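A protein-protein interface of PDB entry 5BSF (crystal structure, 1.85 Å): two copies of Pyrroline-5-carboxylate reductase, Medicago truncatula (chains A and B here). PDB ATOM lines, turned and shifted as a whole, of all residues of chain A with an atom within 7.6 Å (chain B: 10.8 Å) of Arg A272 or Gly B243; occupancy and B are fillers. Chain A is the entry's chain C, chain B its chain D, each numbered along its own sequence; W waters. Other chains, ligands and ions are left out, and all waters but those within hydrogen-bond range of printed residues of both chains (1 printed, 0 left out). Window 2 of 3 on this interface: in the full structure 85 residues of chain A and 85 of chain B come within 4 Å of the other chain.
The backbone carbonyl oxygen (O) of Gly B243 sits at hydrogen-bond distance from the guanidinium group (NH2) of Arg A272 (2.7 Å).
The side-chain carboxylate (OD1) of Asp A176 is in hydrogen-bond range of the side-chain hydroxyl (OG) of Ser A273 (2.7 Å). NH1 of Arg A272 is in salt-bridge range of OE1 of Glu A275 (3.2 Å).
Among the printed residues, pairs that only touch across the chains: Thr A179 with Thr B245, Ala A268 with Glu B252, Ala A269 with Thr B245, Ala A270 with Ala B203, Arg A272 with Gly B244, Arg A272 with Thr B245, Arg A272 with Ala B248 and Ser A273 with Thr B245.
Of the printed residues of chain A, Gly B243 touches Arg A272 (2.7 Å). Ala A268 touches just one residue of chain B: Glu B252 (3.6 Å). Ala A269 touches just one residue of chain B: Thr B245 (3.3 Å). Of the printed residues of chain B, Ala A270 touches Ala B203 (3.9 Å). Printed residues of chain B within 4 Å of Ser A273: Thr B245. No residue of chain B comes within 4 Å of Glu A275. No residue of chain B comes within 4 Å of Leu A276. Of the printed residues of chain B, Thr A179 touches Thr B245 (3.8 Å). Printed residues of chain A within 4 Å of Thr B245: Thr A179, Ala A269, Arg A272 and Ser A273. Thr B246 touches none of the printed residues of chain A. The nearest printed residue of chain B that does not touch Arg A272 is Pro B242 (5.7 Å). The nearest printed residue of chain A that does not touch Gly B243 is Leu A276 (4.1 Å). The nearest printed residue of chain A that does not touch Glu B252 is Ala A269 (6.1 Å).
Hydrophobic or aromatic side chains of chain A that line the printed part of chain B: Ala A268, Ala A269 and Ala A270. Hydrophobic or aromatic side chains of chain B that line the printed part of chain A: Ala B203 and Ala B248. Among the printed residues, 9 pairs touch across the chains. Among the printed residues, no Asp or Glu carboxylate lies within 4 Å of a Lys or Arg side-chain nitrogen of the other chain.
No position is printed for both chains. Of the 9 pairs that touch across the chains among the printed residues, none has its exchanged pair printed and touching as well.
Water W1 lies within hydrogen-bond range of the backbone carbonyl oxygen (O) of Gly B244 (2.7 Å), the backbone carbonyl oxygen (O) of Gly B243 (2.8 Å) and the guanidinium group (NE) of Arg A272 (3.0 Å).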
ATOM      1  N   ASP A 176     -11.926  32.150  -6.123  1.00  0.00           N
ATOM      2  CA  ASP A 176     -11.407  30.759  -6.406  1.00  0.00           C
ATOM      3  C   ASP A 176     -11.602  29.718  -5.338  1.00  0.00           C
ATOM      4  O   ASP A 176     -12.093  28.590  -5.580  1.00  0.00           O
ATOM      5  CB  ASP A 176      -9.930  30.773  -6.754  1.00  0.00           C
ATOM      6  CG  ASP A 176      -9.683  31.441  -8.076  1.00  0.00           C
ATOM      7  OD1 ASP A 176     -10.490  31.293  -8.993  1.00  0.00           O
ATOM      8  OD2 ASP A 176      -8.683  32.150  -8.144  1.00  0.00           O
ATOM      9  N   THR A 179     -15.235  28.946  -4.884  1.00  0.00           N
ATOM     10  CA  THR A 179     -15.687  28.071  -5.996  1.00  0.00           C
ATOM     11  C   THR A 179     -15.385  26.591  -5.637  1.00  0.00           C
ATOM     12  O   THR A 179     -16.187  25.735  -5.862  1.00  0.00           O
ATOM     13  CB  THR A 179     -15.009  28.491  -7.328  1.00  0.00           C
ATOM     14  OG1 THR A 179     -15.401  29.827  -7.634  1.00  0.00           O
ATOM     15  CG2 THR A 179     -15.427  27.583  -8.456  1.00  0.00           C
ATOM     16  N   VAL A 266     -11.379  20.251  -1.604  1.00  0.00           N
ATOM     17  CA  VAL A 266     -11.536  21.686  -1.624  1.00  0.00           C
ATOM     18  C   VAL A 266     -10.285  22.340  -2.199  1.00  0.00           C
ATOM     19  O   VAL A 266     -10.385  23.232  -3.092  1.00  0.00           O
ATOM     20  CB  VAL A 266     -11.857  22.314  -0.251  1.00  0.00           C
ATOM     21  CG1 VAL A 266     -11.946  23.816  -0.349  1.00  0.00           C
ATOM     22  CG2 VAL A 266     -13.165  21.732   0.258  1.00  0.00           C
ATOM     23  N   VAL A 267      -9.137  21.975  -1.680  1.00  0.00           N
ATOM     24  CA  VAL A 267      -7.872  22.533  -2.158  1.00  0.00           C
ATOM     25  C   VAL A 267      -7.637  22.294  -3.681  1.00  0.00           C
ATOM     26  O   VAL A 267      -7.221  23.224  -4.424  1.00  0.00           O
ATOM     27  CB  VAL A 267      -6.703  22.052  -1.310  1.00  0.00           C
ATOM     28  CG1 VAL A 267      -5.371  22.441  -1.929  1.00  0.00           C
ATOM     29  CG2 VAL A 267      -6.795  22.719   0.054  1.00  0.00           C
ATOM     30  N   ALA A 268      -7.848  21.051  -4.157  1.00  0.00           N
ATOM     31  CA  ALA A 268      -7.693  20.756  -5.550  1.00  0.00           C
ATOM     32  C   ALA A 268      -8.674  21.511  -6.454  1.00  0.00           C
ATOM     33  O   ALA A 268      -8.294  22.069  -7.510  1.00  0.00           O
ATOM     34  CB  ALA A 268      -7.850  19.304  -5.822  1.00  0.00           C
ATOM     35  N   ALA A 269      -9.930  21.550  -6.033  1.00  0.00           N
ATOM     36  CA  ALA A 269     -10.928  22.358  -6.758  1.00  0.00           C
ATOM     37  C   ALA A 269     -10.593  23.862  -6.821  1.00  0.00           C
ATOM     38  O   ALA A 269     -10.729  24.533  -7.853  1.00  0.00           O
ATOM     39  CB  ALA A 269     -12.283  22.149  -6.165  1.00  0.00           C
ATOM     40  N   ALA A 270     -10.137  24.397  -5.703  1.00  0.00           N
ATOM     41  CA  ALA A 270      -9.701  25.818  -5.687  1.00  0.00           C
ATOM     42  C   ALA A 270      -8.497  26.102  -6.587  1.00  0.00           C
ATOM     43  O   ALA A 270      -8.453  27.162  -7.269  1.00  0.00           O
ATOM     44  CB  ALA A 270      -9.402  26.294  -4.243  1.00  0.00           C
ATOM     45  N   LYS A 271      -7.533  25.216  -6.560  1.00  0.00           N
ATOM     46  CA  LYS A 271      -6.384  25.328  -7.418  1.00  0.00           C
ATOM     47  C   LYS A 271      -6.803  25.268  -8.911  1.00  0.00           C
ATOM     48  O   LYS A 271      -6.309  26.040  -9.754  1.00  0.00           O
ATOM     49  CB  LYS A 271      -5.427  24.243  -7.117  1.00  0.00           C
ATOM     50  CG  LYS A 271      -4.216  24.210  -8.047  1.00  0.00           C
ATOM     51  CD  LYS A 271      -3.132  23.233  -7.596  1.00  0.00           C
ATOM     52  CE  LYS A 271      -2.005  23.163  -8.605  1.00  0.00           C
ATOM     53  NZ  LYS A 271      -1.453  21.784  -8.546  1.00  0.00           N
ATOM     54  N   ARG A 272      -7.706  24.365  -9.223  1.00  0.00           N
ATOM     55  CA  ARG A 272      -8.233  24.275 -10.583  1.00  0.00           C
ATOM     56  C   ARG A 272      -8.944  25.571 -11.000  1.00  0.00           C
ATOM     57  O   ARG A 272      -8.789  26.047 -12.124  1.00  0.00           O
ATOM     58  CB  ARG A 272      -9.144  23.090 -10.711  1.00  0.00           C
ATOM     59  CG  ARG A 272      -9.617  22.845 -12.130  1.00  0.00           C
ATOM     60  CD  ARG A 272      -8.465  22.607 -13.081  1.00  0.00           C
ATOM     61  NE  ARG A 272      -8.944  22.207 -14.411  1.00  0.00           N
ATOM     62  CZ  ARG A 272      -8.363  22.481 -15.587  1.00  0.00           C
ATOM     63  NH1 ARG A 272      -7.267  23.258 -15.666  1.00  0.00           N
ATOM     64  NH2 ARG A 272      -8.963  22.027 -16.718  1.00  0.00           N
ATOM     65  N   SER A 273      -9.701  26.144 -10.068  1.00  0.00           N
ATOM     66  CA  SER A 273     -10.400  27.415 -10.318  1.00  0.00           C
ATOM     67  C   SER A 273      -9.369  28.502 -10.715  1.00  0.00           C
ATOM     68  O   SER A 273      -9.542  29.226 -11.675  1.00  0.00           O
ATOM     69  CB  SER A 273     -11.189  27.857  -9.126  1.00  0.00           C
ATOM     70  OG  SER A 273     -11.919  29.024  -9.356  1.00  0.00           O
ATOM     71  N   GLN A 274      -8.306  28.554  -9.946  1.00  0.00           N
ATOM     72  CA  GLN A 274      -7.234  29.536 -10.203  1.00  0.00           C
ATOM     73  C   GLN A 274      -6.582  29.255 -11.564  1.00  0.00           C
ATOM     74  O   GLN A 274      -6.356  30.167 -12.361  1.00  0.00           O
ATOM     75  CB  GLN A 274      -6.194  29.494  -9.058  1.00  0.00           C
ATOM     76  CG  GLN A 274      -5.194  30.604  -9.115  1.00  0.00           C
ATOM     77  CD  GLN A 274      -4.190  30.408 -10.240  1.00  0.00           C
ATOM     78  OE1 GLN A 274      -3.652  29.313 -10.453  1.00  0.00           O
ATOM     79  NE2 GLN A 274      -3.875  31.506 -10.939  1.00  0.00           N
ATOM     80  N   GLU A 275      -6.328  28.006 -11.880  1.00  0.00           N
ATOM     81  CA  GLU A 275      -5.730  27.660 -13.128  1.00  0.00           C
ATOM     82  C   GLU A 275      -6.635  27.995 -14.309  1.00  0.00           C
ATOM     83  O   GLU A 275      -6.141  28.217 -15.361  1.00  0.00           O
ATOM     84  CB  GLU A 275      -5.485  26.185 -13.276  1.00  0.00           C
ATOM     85  CG  GLU A 275      -4.403  25.636 -12.442  1.00  0.00           C
ATOM     86  CD  GLU A 275      -4.358  24.097 -12.526  1.00  0.00           C
ATOM     87  OE1 GLU A 275      -5.125  23.423 -13.317  1.00  0.00           O
ATOM     88  OE2 GLU A 275      -3.523  23.630 -11.783  1.00  0.00           O
ATOM     89  N   LEU A 276      -7.942  27.939 -14.143  1.00  0.00           N
ATOM     90  CA  LEU A 276      -8.876  28.239 -15.221  1.00  0.00           C
ATOM     91  C   LEU A 276      -9.135  29.745 -15.384  1.00  0.00           C
ATOM     92  O   LEU A 276      -9.835  30.095 -16.273  1.00  0.00           O
ATOM     93  CB  LEU A 276     -10.251  27.551 -14.995  1.00  0.00           C
ATOM     94  CG  LEU A 276     -10.208  26.019 -15.121  1.00  0.00           C
ATOM     95  CD1 LEU A 276     -11.477  25.416 -14.621  1.00  0.00           C
ATOM     96  CD2 LEU A 276      -9.949  25.660 -16.578  1.00  0.00           C
ATOM     97  N   SER A 277      -8.617  30.581 -14.493  1.00  0.00           N
ATOM     98  CA  SER A 277      -9.042  31.952 -14.310  1.00  0.00           C
ATOM     99  C   SER A 277      -8.359  32.806 -15.381  1.00  0.00           C
ATOM    100  O   SER A 277      -7.382  32.439 -16.028  1.00  0.00           O
ATOM    101  CB  SER A 277      -8.655  32.505 -12.924  1.00  0.00           C
ATOM    102  OG  SER A 277      -7.238  32.638 -12.794  1.00  0.00           O
ATOM    103  OXT SER A 277      -8.853  33.887 -15.594  1.00  0.00           O
ATOM    104  N   ALA B 203      -7.370  26.795   1.603  1.00  0.00           N
ATOM    105  CA  ALA B 203      -7.358  27.433   0.341  1.00  0.00           C
ATOM    106  C   ALA B 203      -7.326  28.941   0.404  1.00  0.00           C
ATOM    107  O   ALA B 203      -7.509  29.603  -0.632  1.00  0.00           O
ATOM    108  CB  ALA B 203      -8.527  26.921  -0.501  1.00  0.00           C
ATOM    109  N   ASP B 237     -23.400  14.250 -11.861  1.00  0.00           N
ATOM    110  CA  ASP B 237     -23.174  14.528 -13.268  1.00  0.00           C
ATOM    111  C   ASP B 237     -23.590  15.932 -13.645  1.00  0.00           C
ATOM    112  O   ASP B 237     -22.903  16.605 -14.410  1.00  0.00           O
ATOM    113  CB  ASP B 237     -23.893  13.514 -14.148  1.00  0.00           C
ATOM    114  CG  ASP B 237     -23.225  12.166 -14.099  1.00  0.00           C
ATOM    115  OD1 ASP B 237     -22.166  11.992 -13.481  1.00  0.00           O
ATOM    116  OD2 ASP B 237     -23.663  11.216 -14.790  1.00  0.00           O
ATOM    117  N   VAL B 239     -23.341  18.648 -12.049  1.00  0.00           N
ATOM    118  CA  VAL B 239     -22.460  19.726 -11.584  1.00  0.00           C
ATOM    119  C   VAL B 239     -21.015  19.539 -12.002  1.00  0.00           C
ATOM    120  O   VAL B 239     -20.200  20.363 -11.677  1.00  0.00           O
ATOM    121  CB  VAL B 239     -22.549  19.959 -10.038  1.00  0.00           C
ATOM    122  CG1 VAL B 239     -23.953  20.430  -9.679  1.00  0.00           C
ATOM    123  CG2 VAL B 239     -22.242  18.703  -9.225  1.00  0.00           C
ATOM    124  N   THR B 240     -20.667  18.415 -12.602  1.00  0.00           N
ATOM    125  CA  THR B 240     -19.265  18.172 -12.937  1.00  0.00           C
ATOM    126  C   THR B 240     -18.973  18.589 -14.369  1.00  0.00           C
ATOM    127  O   THR B 240     -18.918  17.791 -15.303  1.00  0.00           O
ATOM    128  CB  THR B 240     -18.835  16.724 -12.729  1.00  0.00           C
ATOM    129  OG1 THR B 240     -19.882  15.846 -13.153  1.00  0.00           O
ATOM    130  CG2 THR B 240     -18.607  16.451 -11.251  1.00  0.00           C
ATOM    131  N   SER B 241     -18.779  19.874 -14.558  1.00  0.00           N
ATOM    132  CA  SER B 241     -18.548  20.380 -15.895  1.00  0.00           C
ATOM    133  C   SER B 241     -17.186  19.855 -16.406  1.00  0.00           C
ATOM    134  O   SER B 241     -16.240  19.579 -15.658  1.00  0.00           O
ATOM    135  CB  SER B 241     -18.681  21.938 -15.950  1.00  0.00           C
ATOM    136  OG  SER B 241     -17.493  22.443 -15.443  1.00  0.00           O
ATOM    137  N   PRO B 242     -17.053  19.673 -17.721  1.00  0.00           N
ATOM    138  CA  PRO B 242     -15.811  19.133 -18.306  1.00  0.00           C
ATOM    139  C   PRO B 242     -14.550  19.812 -17.887  1.00  0.00           C
ATOM    140  O   PRO B 242     -14.384  20.990 -18.055  1.00  0.00           O
ATOM    141  CB  PRO B 242     -15.996  19.338 -19.833  1.00  0.00           C
ATOM    142  CG  PRO B 242     -17.501  19.334 -20.007  1.00  0.00           C
ATOM    143  CD  PRO B 242     -18.077  19.994 -18.765  1.00  0.00           C
ATOM    144  N   GLY B 243     -13.592  19.045 -17.423  1.00  0.00           N
ATOM    145  CA  GLY B 243     -12.313  19.563 -16.943  1.00  0.00           C
ATOM    146  C   GLY B 243     -12.378  20.674 -15.862  1.00  0.00           C
ATOM    147  O   GLY B 243     -11.433  21.407 -15.684  1.00  0.00           O
ATOM    148  N   GLY B 244     -13.495  20.811 -15.173  1.00  0.00           N
ATOM    149  CA  GLY B 244     -13.738  21.894 -14.295  1.00  0.00           C
ATOM    150  C   GLY B 244     -13.232  21.717 -12.853  1.00  0.00           C
ATOM    151  O   GLY B 244     -12.628  20.686 -12.480  1.00  0.00           O
ATOM    152  N   THR B 245     -13.649  22.642 -12.017  1.00  0.00           N
ATOM    153  CA  THR B 245     -13.233  22.619 -10.622  1.00  0.00           C
ATOM    154  C   THR B 245     -13.860  21.436  -9.854  1.00  0.00           C
ATOM    155  O   THR B 245     -13.241  20.788  -9.036  1.00  0.00           O
ATOM    156  CB  THR B 245     -13.547  23.927  -9.967  1.00  0.00           C
ATOM    157  OG1 THR B 245     -14.953  24.133  -9.856  1.00  0.00           O
ATOM    158  CG2 THR B 245     -12.972  25.045 -10.714  1.00  0.00           C
ATOM    159  N   THR B 246     -15.111  21.158 -10.165  1.00  0.00           N
ATOM    160  CA  THR B 246     -15.860  20.135  -9.458  1.00  0.00           C
ATOM    161  C   THR B 246     -15.322  18.777  -9.677  1.00  0.00           C
ATOM    162  O   THR B 246     -15.086  18.022  -8.681  1.00  0.00           O
ATOM    163  CB  THR B 246     -17.350  20.241  -9.739  1.00  0.00           C
ATOM    164  OG1 THR B 246     -17.769  21.583  -9.529  1.00  0.00           O
ATOM    165  CG2 THR B 246     -18.128  19.353  -8.858  1.00  0.00           C
ATOM    166  N   ILE B 247     -15.049  18.412 -10.933  1.00  0.00           N
ATOM    167  CA  ILE B 247     -14.471  17.092 -11.212  1.00  0.00           C
ATOM    168  C   ILE B 247     -13.088  16.965 -10.632  1.00  0.00           C
ATOM    169  O   ILE B 247     -12.672  15.904 -10.247  1.00  0.00           O
ATOM    170  CB  ILE B 247     -14.545  16.697 -12.696  1.00  0.00           C
ATOM    171  CG1 ILE B 247     -14.287  15.208 -12.906  1.00  0.00           C
ATOM    172  CG2 ILE B 247     -13.588  17.573 -13.519  1.00  0.00           C
ATOM    173  CD1 ILE B 247     -15.405  14.322 -12.363  1.00  0.00           C
ATOM    174  N   ALA B 248     -12.343  18.072 -10.573  1.00  0.00           N
ATOM    175  CA  ALA B 248     -11.026  18.010  -9.896  1.00  0.00           C
ATOM    176  C   ALA B 248     -11.138  17.607  -8.420  1.00  0.00           C
ATOM    177  O   ALA B 248     -10.385  16.774  -7.932  1.00  0.00           O
ATOM    178  CB  ALA B 248     -10.241  19.320 -10.026  1.00  0.00           C
ATOM    179  N   GLY B 249     -12.087  18.168  -7.729  1.00  0.00           N
ATOM    180  CA  GLY B 249     -12.305  17.789  -6.340  1.00  0.00           C
ATOM    181  C   GLY B 249     -12.885  16.401  -6.172  1.00  0.00           C
ATOM    182  O   GLY B 249     -12.411  15.622  -5.353  1.00  0.00           O
ATOM    183  N   VAL B 250     -13.795  16.037  -7.074  1.00  0.00           N
ATOM    184  CA  VAL B 250     -14.341  14.667  -7.027  1.00  0.00           C
ATOM    185  C   VAL B 250     -13.262  13.621  -7.298  1.00  0.00           C
ATOM    186  O   VAL B 250     -13.226  12.572  -6.672  1.00  0.00           O
ATOM    187  CB  VAL B 250     -15.488  14.527  -8.068  1.00  0.00           C
ATOM    188  CG1 VAL B 250     -15.855  13.076  -8.283  1.00  0.00           C
ATOM    189  CG2 VAL B 250     -16.692  15.295  -7.581  1.00  0.00           C
ATOM    190  N   HIS B 251     -12.339  13.921  -8.222  1.00  0.00           N
ATOM    191  CA  HIS B 251     -11.294  12.980  -8.530  1.00  0.00           C
ATOM    192  C   HIS B 251     -10.448  12.769  -7.267  1.00  0.00           C
ATOM    193  O   HIS B 251     -10.048  11.614  -6.986  1.00  0.00           O
ATOM    194  CB  HIS B 251     -10.471  13.488  -9.696  1.00  0.00           C
ATOM    195  CG  HIS B 251      -9.529  12.489 -10.264  1.00  0.00           C
ATOM    196  ND1 HIS B 251      -8.621  12.821 -11.228  1.00  0.00           N
ATOM    197  CD2 HIS B 251      -9.305  11.177  -9.973  1.00  0.00           C
ATOM    198  CE1 HIS B 251      -7.892  11.759 -11.529  1.00  0.00           C
ATOM    199  NE2 HIS B 251      -8.293  10.744 -10.784  1.00  0.00           N
ATOM    200  N   GLU B 252     -10.208  13.821  -6.496  1.00  0.00           N
ATOM    201  CA  GLU B 252      -9.404  13.616  -5.255  1.00  0.00           C
ATOM    202  C   GLU B 252     -10.145  12.704  -4.292  1.00  0.00           C
ATOM    203  O   GLU B 252      -9.556  11.876  -3.640  1.00  0.00           O
ATOM    204  CB  GLU B 252      -9.041  14.932  -4.575  1.00  0.00           C
ATOM    205  CG  GLU B 252      -8.004  15.766  -5.310  1.00  0.00           C
ATOM    206  CD  GLU B 252      -6.660  15.036  -5.510  1.00  0.00           C
ATOM    207  OE1 GLU B 252      -6.169  14.529  -4.492  1.00  0.00           O
ATOM    208  OE2 GLU B 252      -6.349  14.902  -6.692  1.00  0.00           O
HETATM  209  O   HOH W   1     -10.384  19.682 -13.708  1.00  0.00           O
